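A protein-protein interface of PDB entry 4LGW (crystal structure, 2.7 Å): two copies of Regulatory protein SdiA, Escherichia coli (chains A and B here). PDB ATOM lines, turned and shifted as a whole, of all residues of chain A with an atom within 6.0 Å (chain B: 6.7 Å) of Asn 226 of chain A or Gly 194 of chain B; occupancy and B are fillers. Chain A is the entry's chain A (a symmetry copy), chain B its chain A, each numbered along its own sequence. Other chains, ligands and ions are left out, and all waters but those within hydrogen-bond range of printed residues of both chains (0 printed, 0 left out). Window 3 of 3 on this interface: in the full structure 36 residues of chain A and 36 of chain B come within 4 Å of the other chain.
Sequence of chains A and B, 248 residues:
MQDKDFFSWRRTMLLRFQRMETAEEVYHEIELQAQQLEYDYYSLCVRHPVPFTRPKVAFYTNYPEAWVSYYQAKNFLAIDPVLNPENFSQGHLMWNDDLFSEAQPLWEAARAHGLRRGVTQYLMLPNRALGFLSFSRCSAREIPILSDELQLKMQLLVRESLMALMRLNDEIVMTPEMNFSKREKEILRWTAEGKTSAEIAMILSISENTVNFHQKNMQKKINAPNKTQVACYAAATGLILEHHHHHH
The backbone carbonyl oxygen (O) of Glu 193 of chain B lies close to the side-chain amide oxygen (OE1) of Gln 229 of chain A (2.9 Å). OD1 of Asn 226 of chain A lies close to O of Gly 194 of chain B. OG1 of Thr 228 of chain A is in hydrogen-bond range of O of Thr 191 of chain B (3.5 Å).
The side-chain amide nitrogen (ND2) of Asn 226 of chain A sits close to the backbone NH (N) of Thr 228 of chain A, at 3.1 Å. The side-chain amide nitrogen (ND2) of Asn 226 of chain A sits close to the backbone NH (N) of Gln 229 of chain A (2.9 Å).
CA of Gln 229 of chain A touches O of Ala 192 of chain B, 3.4 Å away. Gln 229 of chain A touches Gly 194 of chain B (CB to CA, 3.9 Å).
Of chain B, only Gly 194 comes within 4 Å of Asn 226 of chain A. Gly 194 of chain B touches just these residues of chain A: Asn 226 (2.8 Å) and Gln 229 (3.9 Å). Printed residues of chain A within 4 Å of Ala 192 of chain B: Gln 229. Printed residues of chain A within 4 Å of Glu 193 of chain B: Gln 229 (2.9 Å). Of the printed residues of chain A, Thr 191 of chain B touches Thr 228. Thr 196 of chain B touches none of the printed residues of chain A. Ala 231 of chain A touches none of the printed residues of chain B. The nearest residue of chain B that does not touch Asn 226 of chain A is Lys 195 of chain B (4.7 Å). The nearest printed residue of chain B that does not touch Thr 228 of chain A is Ala 192 of chain B (4.3 Å).
Printed residues of chain B that touch a printed residue of chain A: Thr 191, Ala 192, Glu 193 and Gly 194. Among the printed residues, 5 pairs touch across the chains.
Position printed for both chains: 227. Of the 5 pairs that touch across the chains among the printed residues, none has its exchanged pair printed and touching as well.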
ATOM      1  N   GLN A 219      22.049 -10.572  -2.957  1.00  0.00           N
ATOM      2  CA  GLN A 219      21.695 -10.134  -1.612  1.00  0.00           C
ATOM      3  C   GLN A 219      22.272 -11.045  -0.537  1.00  0.00           C
ATOM      4  O   GLN A 219      22.698 -10.568   0.510  1.00  0.00           O
ATOM      5  CB  GLN A 219      20.184 -10.034  -1.457  1.00  0.00           C
ATOM      6  CG  GLN A 219      19.586  -8.971  -2.332  1.00  0.00           C
ATOM      7  CD  GLN A 219      18.091  -9.041  -2.435  1.00  0.00           C
ATOM      8  OE1 GLN A 219      17.548  -9.007  -3.534  1.00  0.00           O
ATOM      9  NE2 GLN A 219      17.411  -9.138  -1.294  1.00  0.00           N
ATOM     10  N   ALA A 224      22.270  -8.129   2.049  1.00  0.00           N
ATOM     11  CA  ALA A 224      21.483  -6.926   1.839  1.00  0.00           C
ATOM     12  C   ALA A 224      19.984  -7.229   1.846  1.00  0.00           C
ATOM     13  O   ALA A 224      19.573  -8.292   1.390  1.00  0.00           O
ATOM     14  CB  ALA A 224      21.876  -6.302   0.521  1.00  0.00           C
ATOM     15  N   PRO A 225      19.156  -6.276   2.312  1.00  0.00           N
ATOM     16  CA  PRO A 225      17.717  -6.518   2.442  1.00  0.00           C
ATOM     17  C   PRO A 225      17.023  -6.647   1.097  1.00  0.00           C
ATOM     18  O   PRO A 225      16.127  -7.474   0.967  1.00  0.00           O
ATOM     19  CB  PRO A 225      17.193  -5.260   3.153  1.00  0.00           C
ATOM     20  CG  PRO A 225      18.386  -4.534   3.639  1.00  0.00           C
ATOM     21  CD  PRO A 225      19.507  -4.901   2.704  1.00  0.00           C
ATOM     22  N   ASN A 226      17.434  -5.836   0.111  1.00  0.00           N
ATOM     23  CA  ASN A 226      16.775  -5.756  -1.209  1.00  0.00           C
ATOM     24  C   ASN A 226      17.723  -5.431  -2.381  1.00  0.00           C
ATOM     25  O   ASN A 226      18.904  -5.081  -2.179  1.00  0.00           O
ATOM     26  CB  ASN A 226      15.676  -4.712  -1.159  1.00  0.00           C
ATOM     27  CG  ASN A 226      16.158  -3.400  -0.583  1.00  0.00           C
ATOM     28  OD1 ASN A 226      15.645  -2.932   0.430  1.00  0.00           O
ATOM     29  ND2 ASN A 226      17.164  -2.807  -1.213  1.00  0.00           N
ATOM     30  N   LYS A 227      17.198  -5.506  -3.607  1.00  0.00           N
ATOM     31  CA  LYS A 227      18.014  -5.215  -4.804  1.00  0.00           C
ATOM     32  C   LYS A 227      18.594  -3.789  -4.795  1.00  0.00           C
ATOM     33  O   LYS A 227      19.688  -3.524  -5.288  1.00  0.00           O
ATOM     34  CB  LYS A 227      17.202  -5.456  -6.085  1.00  0.00           C
ATOM     35  CG  LYS A 227      16.052  -4.488  -6.290  1.00  0.00           C
ATOM     36  CD  LYS A 227      15.026  -5.034  -7.258  1.00  0.00           C
ATOM     37  CE  LYS A 227      14.135  -3.888  -7.773  1.00  0.00           C
ATOM     38  NZ  LYS A 227      13.552  -4.217  -9.132  1.00  0.00           N
ATOM     39  N   THR A 228      17.848  -2.875  -4.209  1.00  0.00           N
ATOM     40  CA  THR A 228      18.203  -1.486  -4.300  1.00  0.00           C
ATOM     41  C   THR A 228      19.450  -1.157  -3.470  1.00  0.00           C
ATOM     42  O   THR A 228      20.293  -0.378  -3.909  1.00  0.00           O
ATOM     43  CB  THR A 228      16.936  -0.518  -4.221  1.00  0.00           C
ATOM     44  OG1 THR A 228      17.171   0.562  -3.315  1.00  0.00           O
ATOM     45  CG2 THR A 228      15.639  -1.276  -3.868  1.00  0.00           C
ATOM     46  N   GLN A 229      19.626  -1.803  -2.322  1.00  0.00           N
ATOM     47  CA  GLN A 229      20.889  -1.653  -1.599  1.00  0.00           C
ATOM     48  C   GLN A 229      22.032  -2.251  -2.408  1.00  0.00           C
ATOM     49  O   GLN A 229      23.091  -1.641  -2.488  1.00  0.00           O
ATOM     50  CB  GLN A 229      20.873  -2.263  -0.208  1.00  0.00           C
ATOM     51  CG  GLN A 229      22.223  -2.086   0.480  1.00  0.00           C
ATOM     52  CD  GLN A 229      22.352  -2.791   1.823  1.00  0.00           C
ATOM     53  OE1 GLN A 229      21.654  -2.461   2.769  1.00  0.00           O
ATOM     54  NE2 GLN A 229      23.267  -3.743   1.914  1.00  0.00           N
ATOM     55  N   VAL A 230      21.831  -3.423  -3.009  1.00  0.00           N
ATOM     56  CA  VAL A 230      22.867  -4.020  -3.841  1.00  0.00           C
ATOM     57  C   VAL A 230      23.294  -3.062  -4.976  1.00  0.00           C
ATOM     58  O   VAL A 230      24.489  -2.726  -5.122  1.00  0.00           O
ATOM     59  CB  VAL A 230      22.434  -5.393  -4.421  1.00  0.00           C
ATOM     60  CG1 VAL A 230      23.544  -6.009  -5.266  1.00  0.00           C
ATOM     61  CG2 VAL A 230      22.049  -6.329  -3.321  1.00  0.00           C
ATOM     62  N   ALA A 231      22.320  -2.613  -5.777  1.00  0.00           N
ATOM     63  CA  ALA A 231      22.620  -1.753  -6.918  1.00  0.00           C
ATOM     64  C   ALA A 231      23.302  -0.470  -6.455  1.00  0.00           C
ATOM     65  O   ALA A 231      24.294  -0.055  -7.065  1.00  0.00           O
ATOM     66  CB  ALA A 231      21.378  -1.443  -7.712  1.00  0.00           C
ATOM     67  N   ARG B 189      19.659   8.522   0.907  1.00  0.00           N
ATOM     68  CA  ARG B 189      20.661   7.691   1.591  1.00  0.00           C
ATOM     69  C   ARG B 189      20.059   6.478   2.294  1.00  0.00           C
ATOM     70  O   ARG B 189      20.612   5.364   2.231  1.00  0.00           O
ATOM     71  CB  ARG B 189      21.396   8.515   2.618  1.00  0.00           C
ATOM     72  CG  ARG B 189      22.355   9.471   2.029  1.00  0.00           C
ATOM     73  CD  ARG B 189      23.214  10.043   3.107  1.00  0.00           C
ATOM     74  NE  ARG B 189      22.562  11.141   3.812  1.00  0.00           N
ATOM     75  CZ  ARG B 189      22.495  12.398   3.358  1.00  0.00           C
ATOM     76  NH1 ARG B 189      23.015  12.744   2.174  1.00  0.00           N
ATOM     77  NH2 ARG B 189      21.901  13.324   4.088  1.00  0.00           N
ATOM     78  N   TRP B 190      18.930   6.686   2.978  1.00  0.00           N
ATOM     79  CA  TRP B 190      18.297   5.569   3.661  1.00  0.00           C
ATOM     80  C   TRP B 190      17.750   4.584   2.659  1.00  0.00           C
ATOM     81  O   TRP B 190      17.752   3.367   2.914  1.00  0.00           O
ATOM     82  CB  TRP B 190      17.234   6.021   4.642  1.00  0.00           C
ATOM     83  CG  TRP B 190      17.818   6.705   5.826  1.00  0.00           C
ATOM     84  CD1 TRP B 190      17.798   8.039   6.081  1.00  0.00           C
ATOM     85  CD2 TRP B 190      18.519   6.097   6.912  1.00  0.00           C
ATOM     86  NE1 TRP B 190      18.433   8.310   7.265  1.00  0.00           N
ATOM     87  CE2 TRP B 190      18.886   7.133   7.802  1.00  0.00           C
ATOM     88  CE3 TRP B 190      18.872   4.770   7.229  1.00  0.00           C
ATOM     89  CZ2 TRP B 190      19.607   6.894   8.988  1.00  0.00           C
ATOM     90  CZ3 TRP B 190      19.577   4.522   8.408  1.00  0.00           C
ATOM     91  CH2 TRP B 190      19.942   5.585   9.275  1.00  0.00           C
ATOM     92  N   THR B 191      17.313   5.095   1.511  1.00  0.00           N
ATOM     93  CA  THR B 191      16.895   4.238   0.414  1.00  0.00           C
ATOM     94  C   THR B 191      18.055   3.405  -0.110  1.00  0.00           C
ATOM     95  O   THR B 191      17.908   2.210  -0.351  1.00  0.00           O
ATOM     96  CB  THR B 191      16.330   5.064  -0.726  1.00  0.00           C
ATOM     97  OG1 THR B 191      15.282   5.883  -0.203  1.00  0.00           O
ATOM     98  CG2 THR B 191      15.799   4.171  -1.842  1.00  0.00           C
ATOM     99  N   ALA B 192      19.207   4.033  -0.292  1.00  0.00           N
ATOM    100  CA  ALA B 192      20.360   3.326  -0.834  1.00  0.00           C
ATOM    101  C   ALA B 192      20.863   2.320   0.201  1.00  0.00           C
ATOM    102  O   ALA B 192      21.486   1.318  -0.129  1.00  0.00           O
ATOM    103  CB  ALA B 192      21.452   4.305  -1.217  1.00  0.00           C
ATOM    104  N   GLU B 193      20.557   2.591   1.460  1.00  0.00           N
ATOM    105  CA  GLU B 193      20.932   1.716   2.536  1.00  0.00           C
ATOM    106  C   GLU B 193      19.918   0.574   2.649  1.00  0.00           C
ATOM    107  O   GLU B 193      20.018  -0.254   3.553  1.00  0.00           O
ATOM    108  CB  GLU B 193      20.986   2.535   3.830  1.00  0.00           C
ATOM    109  CG  GLU B 193      22.068   2.142   4.812  1.00  0.00           C
ATOM    110  CD  GLU B 193      23.440   2.034   4.179  1.00  0.00           C
ATOM    111  OE1 GLU B 193      23.988   0.925   4.110  1.00  0.00           O
ATOM    112  OE2 GLU B 193      23.974   3.066   3.745  1.00  0.00           O
ATOM    113  N   GLY B 194      18.929   0.535   1.750  1.00  0.00           N
ATOM    114  CA  GLY B 194      17.952  -0.559   1.712  1.00  0.00           C
ATOM    115  C   GLY B 194      16.727  -0.436   2.612  1.00  0.00           C
ATOM    116  O   GLY B 194      15.946  -1.388   2.715  1.00  0.00           O
ATOM    117  N   LYS B 195      16.541   0.726   3.246  1.00  0.00           N
ATOM    118  CA  LYS B 195      15.369   1.008   4.089  1.00  0.00           C
ATOM    119  C   LYS B 195      14.084   1.231   3.287  1.00  0.00           C
ATOM    120  O   LYS B 195      14.120   1.874   2.236  1.00  0.00           O
ATOM    121  CB  LYS B 195      15.649   2.225   4.971  1.00  0.00           C
ATOM    122  CG  LYS B 195      16.183   1.882   6.361  1.00  0.00           C
ATOM    123  CD  LYS B 195      17.179   0.697   6.331  1.00  0.00           C
ATOM    124  CE  LYS B 195      17.112  -0.203   7.575  1.00  0.00           C
ATOM    125  NZ  LYS B 195      17.767   0.439   8.746  1.00  0.00           N
ATOM    126  N   THR B 196      12.962   0.698   3.782  1.00  0.00           N
ATOM    127  CA  THR B 196      11.608   0.920   3.221  1.00  0.00           C
ATOM    128  C   THR B 196      11.051   2.294   3.623  1.00  0.00           C
ATOM    129  O   THR B 196      11.576   2.944   4.544  1.00  0.00           O
ATOM    130  CB  THR B 196      10.591  -0.116   3.778  1.00  0.00           C
ATOM    131  OG1 THR B 196      10.458   0.059   5.216  1.00  0.00           O
ATOM    132  CG2 THR B 196      10.992  -1.567   3.393  1.00  0.00           C
ATOM    133  N   GLU B 199      10.079   2.317   7.225  1.00  0.00           N
ATOM    134  CA  GLU B 199      11.275   2.448   8.047  1.00  0.00           C
ATOM    135  C   GLU B 199      11.826   3.864   8.032  1.00  0.00           C
ATOM    136  O   GLU B 199      12.191   4.395   9.084  1.00  0.00           O
ATOM    137  CB  GLU B 199      12.336   1.443   7.614  1.00  0.00           C
ATOM    138  CG  GLU B 199      12.092   0.024   8.117  1.00  0.00           C
ATOM    139  CD  GLU B 199      12.899  -1.038   7.365  1.00  0.00           C
ATOM    140  OE1 GLU B 199      13.571  -0.728   6.334  1.00  0.00           O
ATOM    141  OE2 GLU B 199      12.860  -2.208   7.810  1.00  0.00           O
ATOM    142  N   ILE B 200      11.872   4.489   6.851  1.00  0.00           N
ATOM    143  CA  ILE B 200      12.354   5.876   6.748  1.00  0.00           C
ATOM    144  C   ILE B 200      11.459   6.831   7.572  1.00  0.00           C
ATOM    145  O   ILE B 200      11.962   7.696   8.310  1.00  0.00           O
ATOM    146  CB  ILE B 200      12.558   6.333   5.266  1.00  0.00           C
ATOM    147  CG1 ILE B 200      13.636   5.472   4.603  1.00  0.00           C
ATOM    148  CG2 ILE B 200      12.978   7.785   5.207  1.00  0.00           C
ATOM    149  CD1 ILE B 200      13.625   5.435   3.091  1.00  0.00           C
ATOM    150  N   LYS B 227      12.290   4.917  -7.367  1.00  0.00           N
ATOM    151  CA  LYS B 227      13.302   5.402  -6.406  1.00  0.00           C
ATOM    152  C   LYS B 227      14.700   4.815  -6.671  1.00  0.00           C
ATOM    153  O   LYS B 227      15.730   5.452  -6.453  1.00  0.00           O
ATOM    154  CB  LYS B 227      12.862   5.113  -4.964  1.00  0.00           C
ATOM    155  CG  LYS B 227      12.821   3.639  -4.605  1.00  0.00           C
ATOM    156  CD  LYS B 227      11.954   3.382  -3.393  1.00  0.00           C
ATOM    157  CE  LYS B 227      12.281   1.996  -2.805  1.00  0.00           C
ATOM    158  NZ  LYS B 227      11.950   1.937  -1.327  1.00  0.00           N
